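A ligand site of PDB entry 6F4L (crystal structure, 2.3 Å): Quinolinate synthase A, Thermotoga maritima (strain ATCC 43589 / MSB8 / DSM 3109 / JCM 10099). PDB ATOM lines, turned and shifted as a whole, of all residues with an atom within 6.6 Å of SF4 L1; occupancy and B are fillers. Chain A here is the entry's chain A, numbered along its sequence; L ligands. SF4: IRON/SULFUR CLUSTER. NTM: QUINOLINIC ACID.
SG of Cys 88 binds FE4 of SF4 L1, at 2.3 Å.
An iron atom (FE1) of SF4 L1 is bound by the side-chain sulfur (SG) of Cys 175, at 2.3 Å.
An iron atom (FE2) of SF4 L1 is bound by the side-chain sulfur (SG) of Cys 261 (2.4 Å).
OH of Tyr 28 lies within hydrogen-bond range of N1 of NTM L2 (3.4 Å).
A ring nitrogen (NE2) of His 26 is in hydrogen-bond range of an oxygen (O4) of NTM L2, at 2.7 Å.
The side-chain carboxylate of Glu 202 sits close to the side-chain sulfur of Cys 175, 3.5 Å away.
The backbone NH of Tyr 28 lies within hydrogen-bond range of a ring nitrogen (ND1) of His 26, at 2.9 Å.
N of Cys 261 is in hydrogen-bond range of OE2 of Glu 237 (2.8 Å).
The side-chain sulfur (SG) of Cys 175 sits close to a ring nitrogen (ND1) of His 178.
N of Ala 91 lies close to SG of Cys 88, at 3.7 Å.
OE2 of Glu 202 is in hydrogen-bond range of OH of Tyr 114, at 3.0 Å.
The backbone NH of Val 177 lies close to the side-chain sulfur of Cys 175.
A sulfur (S2) of SF4 L1 lies close to the side-chain carboxylate (OE1) of Glu 202 (3.3 Å).
Merely in contact with SF4 L1: Met 90 (3.6 Å), Pro 176 (3.7 Å), Tyr 28 (3.8 Å) and Val 177 (3.9 Å).
Hydrophobic or aromatic side chains within 4 Å of SF4 L1: Tyr 28, Met 90, Pro 176 and Val 177.
Within 4 Å of SF4 L1: Tyr 28, Cys 88, Met 90, Cys 175, Pro 176, Val 177, Glu 202 and Cys 261.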
ATOM      1  N   HIS A  26     -29.021  25.609   3.674  1.00  0.00           N
ATOM      2  CA  HIS A  26     -28.829  24.340   3.017  1.00  0.00           C
ATOM      3  C   HIS A  26     -27.819  23.516   3.800  1.00  0.00           C
ATOM      4  O   HIS A  26     -26.939  24.085   4.454  1.00  0.00           O
ATOM      5  CB  HIS A  26     -28.342  24.552   1.599  1.00  0.00           C
ATOM      6  CG  HIS A  26     -28.253  23.287   0.808  1.00  0.00           C
ATOM      7  ND1 HIS A  26     -27.133  22.498   0.810  1.00  0.00           N
ATOM      8  CD2 HIS A  26     -29.153  22.688   0.002  1.00  0.00           C
ATOM      9  CE1 HIS A  26     -27.333  21.466   0.018  1.00  0.00           C
ATOM     10  NE2 HIS A  26     -28.553  21.550  -0.483  1.00  0.00           N
ATOM     11  N   TYR A  28     -25.245  22.193   3.022  1.00  0.00           N
ATOM     12  CA  TYR A  28     -23.836  22.390   2.678  1.00  0.00           C
ATOM     13  C   TYR A  28     -23.212  23.676   3.206  1.00  0.00           C
ATOM     14  O   TYR A  28     -22.074  23.987   2.866  1.00  0.00           O
ATOM     15  CB  TYR A  28     -23.625  22.304   1.154  1.00  0.00           C
ATOM     16  CG  TYR A  28     -23.952  20.959   0.559  1.00  0.00           C
ATOM     17  CD1 TYR A  28     -24.105  19.819   1.355  1.00  0.00           C
ATOM     18  CD2 TYR A  28     -24.073  20.815  -0.820  1.00  0.00           C
ATOM     19  CE1 TYR A  28     -24.389  18.584   0.805  1.00  0.00           C
ATOM     20  CE2 TYR A  28     -24.367  19.580  -1.391  1.00  0.00           C
ATOM     21  CZ  TYR A  28     -24.517  18.470  -0.578  1.00  0.00           C
ATOM     22  OH  TYR A  28     -24.806  17.264  -1.151  1.00  0.00           O
ATOM     23  N   VAL A  63     -27.344  28.398  -2.667  1.00  0.00           N
ATOM     24  CA  VAL A  63     -26.895  28.962  -3.953  1.00  0.00           C
ATOM     25  C   VAL A  63     -28.082  29.442  -4.785  1.00  0.00           C
ATOM     26  O   VAL A  63     -29.226  29.055  -4.508  1.00  0.00           O
ATOM     27  CB  VAL A  63     -26.009  27.981  -4.731  1.00  0.00           C
ATOM     28  CG1 VAL A  63     -24.678  27.818  -4.015  1.00  0.00           C
ATOM     29  CG2 VAL A  63     -26.717  26.641  -4.869  1.00  0.00           C
ATOM     30  N   PHE A  65     -29.876  29.154  -7.582  1.00  0.00           N
ATOM     31  CA  PHE A  65     -31.001  28.359  -8.063  1.00  0.00           C
ATOM     32  C   PHE A  65     -31.936  27.922  -6.913  1.00  0.00           C
ATOM     33  O   PHE A  65     -33.148  27.877  -7.096  1.00  0.00           O
ATOM     34  CB  PHE A  65     -30.569  27.148  -8.927  1.00  0.00           C
ATOM     35  CG  PHE A  65     -30.083  25.955  -8.145  1.00  0.00           C
ATOM     36  CD1 PHE A  65     -31.001  25.091  -7.517  1.00  0.00           C
ATOM     37  CD2 PHE A  65     -28.728  25.668  -8.031  1.00  0.00           C
ATOM     38  CE1 PHE A  65     -30.570  24.002  -6.762  1.00  0.00           C
ATOM     39  CE2 PHE A  65     -28.289  24.568  -7.294  1.00  0.00           C
ATOM     40  CZ  PHE A  65     -29.218  23.737  -6.651  1.00  0.00           C
ATOM     41  N   MET A  66     -31.368  27.616  -5.754  1.00  0.00           N
ATOM     42  CA  MET A  66     -32.181  27.196  -4.621  1.00  0.00           C
ATOM     43  C   MET A  66     -33.031  28.362  -4.080  1.00  0.00           C
ATOM     44  O   MET A  66     -34.209  28.190  -3.830  1.00  0.00           O
ATOM     45  CB  MET A  66     -31.330  26.634  -3.501  1.00  0.00           C
ATOM     46  CG  MET A  66     -30.323  25.599  -3.893  1.00  0.00           C
ATOM     47  SD  MET A  66     -29.345  25.091  -2.478  1.00  0.00           S
ATOM     48  CE  MET A  66     -28.529  23.691  -3.243  1.00  0.00           C
ATOM     49  N   THR A  87     -23.573  30.371  -6.889  1.00  0.00           N
ATOM     50  CA  THR A  87     -24.256  29.767  -8.031  1.00  0.00           C
ATOM     51  C   THR A  87     -23.806  28.318  -8.159  1.00  0.00           C
ATOM     52  O   THR A  87     -22.969  27.861  -7.396  1.00  0.00           O
ATOM     53  CB  THR A  87     -24.031  30.594  -9.322  1.00  0.00           C
ATOM     54  OG1 THR A  87     -25.002  30.227 -10.323  1.00  0.00           O
ATOM     55  CG2 THR A  87     -22.584  30.447  -9.890  1.00  0.00           C
ATOM     56  N   CYS A  88     -24.372  27.595  -9.122  1.00  0.00           N
ATOM     57  CA  CYS A  88     -23.960  26.231  -9.375  1.00  0.00           C
ATOM     58  C   CYS A  88     -23.377  26.156 -10.792  1.00  0.00           C
ATOM     59  O   CYS A  88     -24.126  26.302 -11.775  1.00  0.00           O
ATOM     60  CB  CYS A  88     -25.136  25.287  -9.178  1.00  0.00           C
ATOM     61  SG  CYS A  88     -24.745  23.538  -9.405  1.00  0.00           S
ATOM     62  N   PRO A  89     -22.047  25.965 -10.924  1.00  0.00           N
ATOM     63  CA  PRO A  89     -21.434  25.911 -12.268  1.00  0.00           C
ATOM     64  C   PRO A  89     -21.888  24.725 -13.118  1.00  0.00           C
ATOM     65  O   PRO A  89     -21.997  24.872 -14.343  1.00  0.00           O
ATOM     66  CB  PRO A  89     -19.936  25.841 -11.955  1.00  0.00           C
ATOM     67  CG  PRO A  89     -19.820  26.518 -10.631  1.00  0.00           C
ATOM     68  CD  PRO A  89     -21.017  26.004  -9.872  1.00  0.00           C
ATOM     69  N   MET A  90     -22.156  23.574 -12.498  1.00  0.00           N
ATOM     70  CA  MET A  90     -22.773  22.455 -13.194  1.00  0.00           C
ATOM     71  C   MET A  90     -24.079  22.919 -13.887  1.00  0.00           C
ATOM     72  O   MET A  90     -24.173  22.868 -15.121  1.00  0.00           O
ATOM     73  CB  MET A  90     -23.024  21.267 -12.244  1.00  0.00           C
ATOM     74  CG  MET A  90     -23.770  20.105 -12.912  1.00  0.00           C
ATOM     75  SD  MET A  90     -24.599  18.903 -11.822  1.00  0.00           S
ATOM     76  CE  MET A  90     -25.619  19.912 -10.740  1.00  0.00           C
ATOM     77  N   ALA A  91     -25.039  23.416 -13.100  1.00  0.00           N
ATOM     78  CA  ALA A  91     -26.341  23.894 -13.601  1.00  0.00           C
ATOM     79  C   ALA A  91     -26.213  24.872 -14.779  1.00  0.00           C
ATOM     80  O   ALA A  91     -26.908  24.723 -15.786  1.00  0.00           O
ATOM     81  CB  ALA A  91     -27.167  24.519 -12.475  1.00  0.00           C
ATOM     82  N   TYR A 114     -33.191  18.253 -13.408  1.00  0.00           N
ATOM     83  CA  TYR A 114     -32.692  18.209 -12.031  1.00  0.00           C
ATOM     84  C   TYR A 114     -32.875  19.576 -11.404  1.00  0.00           C
ATOM     85  O   TYR A 114     -32.775  20.604 -12.094  1.00  0.00           O
ATOM     86  CB  TYR A 114     -31.206  17.788 -11.998  1.00  0.00           C
ATOM     87  CG  TYR A 114     -30.596  17.562 -10.629  1.00  0.00           C
ATOM     88  CD1 TYR A 114     -31.338  16.975  -9.601  1.00  0.00           C
ATOM     89  CD2 TYR A 114     -29.271  17.916 -10.361  1.00  0.00           C
ATOM     90  CE1 TYR A 114     -30.784  16.752  -8.341  1.00  0.00           C
ATOM     91  CE2 TYR A 114     -28.703  17.691  -9.099  1.00  0.00           C
ATOM     92  CZ  TYR A 114     -29.484  17.109  -8.097  1.00  0.00           C
ATOM     93  OH  TYR A 114     -28.975  16.882  -6.832  1.00  0.00           O
ATOM     94  N   ASN A 116     -31.003  21.310  -9.382  1.00  0.00           N
ATOM     95  CA  ASN A 116     -29.791  22.097  -9.639  1.00  0.00           C
ATOM     96  C   ASN A 116     -29.755  22.412 -11.126  1.00  0.00           C
ATOM     97  O   ASN A 116     -29.054  21.760 -11.891  1.00  0.00           O
ATOM     98  CB  ASN A 116     -28.494  21.378  -9.174  1.00  0.00           C
ATOM     99  N   ASP A 151     -27.029  16.762 -14.635  1.00  0.00           N
ATOM    100  CA  ASP A 151     -26.062  15.824 -14.049  1.00  0.00           C
ATOM    101  C   ASP A 151     -26.129  14.436 -14.687  1.00  0.00           C
ATOM    102  O   ASP A 151     -27.136  13.749 -14.555  1.00  0.00           O
ATOM    103  CB  ASP A 151     -26.267  15.720 -12.525  1.00  0.00           C
ATOM    104  CG  ASP A 151     -25.137  14.959 -11.824  1.00  0.00           C
ATOM    105  OD1 ASP A 151     -25.096  13.704 -11.944  1.00  0.00           O
ATOM    106  OD2 ASP A 151     -24.295  15.602 -11.162  1.00  0.00           O
ATOM    107  N   HIS A 174     -21.445  17.227 -14.647  1.00  0.00           N
ATOM    108  CA  HIS A 174     -21.043  16.585 -13.405  1.00  0.00           C
ATOM    109  C   HIS A 174     -20.829  17.623 -12.307  1.00  0.00           C
ATOM    110  O   HIS A 174     -20.565  18.800 -12.585  1.00  0.00           O
ATOM    111  CB  HIS A 174     -19.767  15.783 -13.634  1.00  0.00           C
ATOM    112  CG  HIS A 174     -18.554  16.629 -13.775  1.00  0.00           C
ATOM    113  ND1 HIS A 174     -18.365  17.487 -14.842  1.00  0.00           N
ATOM    114  CD2 HIS A 174     -17.486  16.795 -12.955  1.00  0.00           C
ATOM    115  CE1 HIS A 174     -17.213  18.129 -14.687  1.00  0.00           C
ATOM    116  NE2 HIS A 174     -16.667  17.732 -13.552  1.00  0.00           N
ATOM    117  N   CYS A 175     -20.970  17.180 -11.074  1.00  0.00           N
ATOM    118  CA  CYS A 175     -20.675  18.001  -9.924  1.00  0.00           C
ATOM    119  C   CYS A 175     -19.278  17.650  -9.403  1.00  0.00           C
ATOM    120  O   CYS A 175     -19.031  16.479  -9.079  1.00  0.00           O
ATOM    121  CB  CYS A 175     -21.732  17.808  -8.855  1.00  0.00           C
ATOM    122  SG  CYS A 175     -21.184  18.240  -7.186  1.00  0.00           S
ATOM    123  N   PRO A 176     -18.382  18.660  -9.298  1.00  0.00           N
ATOM    124  CA  PRO A 176     -16.994  18.403  -8.889  1.00  0.00           C
ATOM    125  C   PRO A 176     -16.858  17.889  -7.451  1.00  0.00           C
ATOM    126  O   PRO A 176     -16.031  17.028  -7.195  1.00  0.00           O
ATOM    127  CB  PRO A 176     -16.316  19.780  -9.033  1.00  0.00           C
ATOM    128  CG  PRO A 176     -17.321  20.676  -9.711  1.00  0.00           C
ATOM    129  CD  PRO A 176     -18.669  20.102  -9.391  1.00  0.00           C
ATOM    130  N   VAL A 177     -17.688  18.397  -6.546  1.00  0.00           N
ATOM    131  CA  VAL A 177     -17.724  17.997  -5.122  1.00  0.00           C
ATOM    132  C   VAL A 177     -17.932  16.491  -4.924  1.00  0.00           C
ATOM    133  O   VAL A 177     -17.409  15.911  -3.976  1.00  0.00           O
ATOM    134  CB  VAL A 177     -18.813  18.795  -4.351  1.00  0.00           C
ATOM    135  CG1 VAL A 177     -18.887  18.377  -2.889  1.00  0.00           C
ATOM    136  CG2 VAL A 177     -18.543  20.289  -4.438  1.00  0.00           C
ATOM    137  N   HIS A 178     -18.675  15.847  -5.816  1.00  0.00           N
ATOM    138  CA  HIS A 178     -19.010  14.428  -5.674  1.00  0.00           C
ATOM    139  C   HIS A 178     -18.149  13.451  -6.477  1.00  0.00           C
ATOM    140  O   HIS A 178     -18.480  12.262  -6.550  1.00  0.00           O
ATOM    141  CB  HIS A 178     -20.511  14.190  -5.936  1.00  0.00           C
ATOM    142  CG  HIS A 178     -21.388  14.735  -4.859  1.00  0.00           C
ATOM    143  ND1 HIS A 178     -22.121  15.897  -5.012  1.00  0.00           N
ATOM    144  CD2 HIS A 178     -21.624  14.307  -3.599  1.00  0.00           C
ATOM    145  CE1 HIS A 178     -22.780  16.146  -3.886  1.00  0.00           C
ATOM    146  NE2 HIS A 178     -22.492  15.189  -3.021  1.00  0.00           N
ATOM    147  N   GLU A 202     -25.082  11.543  -7.222  1.00  0.00           N
ATOM    148  CA  GLU A 202     -24.219  12.365  -8.066  1.00  0.00           C
ATOM    149  C   GLU A 202     -22.792  11.850  -8.203  1.00  0.00           C
ATOM    150  O   GLU A 202     -22.056  12.342  -9.070  1.00  0.00           O
ATOM    151  CB  GLU A 202     -24.172  13.813  -7.559  1.00  0.00           C
ATOM    152  CG  GLU A 202     -25.271  14.694  -8.115  1.00  0.00           C
ATOM    153  CD  GLU A 202     -25.186  16.123  -7.642  1.00  0.00           C
ATOM    154  OE1 GLU A 202     -24.296  16.869  -8.089  1.00  0.00           O
ATOM    155  OE2 GLU A 202     -26.021  16.539  -6.820  1.00  0.00           O
ATOM    156  N   GLU A 237     -20.616  16.559   0.346  1.00  0.00           N
ATOM    157  CA  GLU A 237     -20.045  17.823   0.808  1.00  0.00           C
ATOM    158  C   GLU A 237     -19.967  17.835   2.347  1.00  0.00           C
ATOM    159  O   GLU A 237     -20.867  17.371   3.038  1.00  0.00           O
ATOM    160  CB  GLU A 237     -20.869  18.995   0.257  1.00  0.00           C
ATOM    161  CG  GLU A 237     -20.104  20.258  -0.086  1.00  0.00           C
ATOM    162  CD  GLU A 237     -19.781  21.122   1.124  1.00  0.00           C
ATOM    163  OE1 GLU A 237     -20.346  20.895   2.219  1.00  0.00           O
ATOM    164  OE2 GLU A 237     -18.983  22.084   0.988  1.00  0.00           O
ATOM    165  N   CYS A 261     -17.752  22.489  -1.499  1.00  0.00           N
ATOM    166  CA  CYS A 261     -18.326  23.318  -2.560  1.00  0.00           C
ATOM    167  C   CYS A 261     -17.901  24.767  -2.338  1.00  0.00           C
ATOM    168  O   CYS A 261     -18.240  25.393  -1.301  1.00  0.00           O
ATOM    169  CB  CYS A 261     -19.865  23.190  -2.615  1.00  0.00           C
ATOM    170  SG  CYS A 261     -20.692  23.910  -4.082  1.00  0.00           S
ATOM    171  N   VAL A 262     -17.135  25.312  -3.288  1.00  0.00           N
ATOM    172  CA  VAL A 262     -16.603  26.681  -3.155  1.00  0.00           C
ATOM    173  C   VAL A 262     -17.751  27.701  -3.054  1.00  0.00           C
ATOM    174  O   VAL A 262     -17.680  28.617  -2.236  1.00  0.00           O
ATOM    175  CB  VAL A 262     -15.665  27.043  -4.327  1.00  0.00           C
ATOM    176  CG1 VAL A 262     -15.113  28.454  -4.177  1.00  0.00           C
ATOM    177  CG2 VAL A 262     -14.513  26.037  -4.430  1.00  0.00           C
ATOM    178  N   ASN A 263     -18.789  27.507  -3.868  1.00  0.00           N
ATOM    179  CA  ASN A 263     -19.938  28.416  -3.907  1.00  0.00           C
ATOM    180  C   ASN A 263     -20.780  28.388  -2.645  1.00  0.00           C
ATOM    181  O   ASN A 263     -21.298  29.426  -2.210  1.00  0.00           O
ATOM    182  CB  ASN A 263     -20.797  28.118  -5.123  1.00  0.00           C
ATOM    183  CG  ASN A 263     -20.324  28.856  -6.343  1.00  0.00           C
ATOM    184  OD1 ASN A 263     -20.521  30.060  -6.471  1.00  0.00           O
ATOM    185  ND2 ASN A 263     -19.686  28.133  -7.271  1.00  0.00           N
ATOM    186  N   MET A 264     -20.931  27.211  -2.058  1.00  0.00           N
ATOM    187  CA  MET A 264     -21.658  27.101  -0.803  1.00  0.00           C
ATOM    188  C   MET A 264     -20.916  27.835   0.313  1.00  0.00           C
ATOM    189  O   MET A 264     -21.527  28.412   1.208  1.00  0.00           O
ATOM    190  CB  MET A 264     -21.872  25.628  -0.468  1.00  0.00           C
ATOM    191  CG  MET A 264     -22.974  25.011  -1.308  1.00  0.00           C
ATOM    192  SD  MET A 264     -24.600  25.546  -0.692  1.00  0.00           S
ATOM    193  CE  MET A 264     -25.633  24.578  -1.771  1.00  0.00           C
HETATM  194 FE1  SF4 L   1     -22.347  20.162  -6.682  1.00  0.00          FE
HETATM  195 FE2  SF4 L   1     -22.053  22.793  -5.645  1.00  0.00          FE
HETATM  196 FE3  SF4 L   1     -24.440  21.343  -5.310  1.00  0.00          FE
HETATM  197 FE4  SF4 L   1     -23.651  22.233  -7.863  1.00  0.00          FE
HETATM  198  S1  SF4 L   1     -24.161  23.615  -6.003  1.00  0.00           S
HETATM  199  S2  SF4 L   1     -24.543  20.002  -7.255  1.00  0.00           S
HETATM  200  S3  SF4 L   1     -21.380  22.042  -7.812  1.00  0.00           S
HETATM  201  S4  SF4 L   1     -22.372  20.853  -4.394  1.00  0.00           S
HETATM  202  N1  NTM L   2     -27.403  17.419  -3.349  1.00  0.00           N
HETATM  203  C2  NTM L   2     -28.596  17.804  -2.854  1.00  0.00           C
HETATM  204  C3  NTM L   2     -29.171  19.099  -3.304  1.00  0.00           C
HETATM  205  C4  NTM L   2     -28.440  19.836  -4.206  1.00  0.00           C
HETATM  206  C5  NTM L   2     -27.224  19.376  -4.660  1.00  0.00           C
HETATM  207  C6  NTM L   2     -26.727  18.162  -4.219  1.00  0.00           C
HETATM  208  C7  NTM L   2     -29.259  16.887  -1.863  1.00  0.00           C
HETATM  209  O1  NTM L   2     -28.744  15.792  -1.624  1.00  0.00           O
HETATM  210  O2  NTM L   2     -30.302  17.239  -1.294  1.00  0.00           O
HETATM  211  C8  NTM L   2     -30.464  19.655  -2.839  1.00  0.00           C
HETATM  212  O3  NTM L   2     -31.478  19.330  -3.403  1.00  0.00           O
HETATM  213  O4  NTM L   2     -30.513  20.451  -1.913  1.00  0.00           O
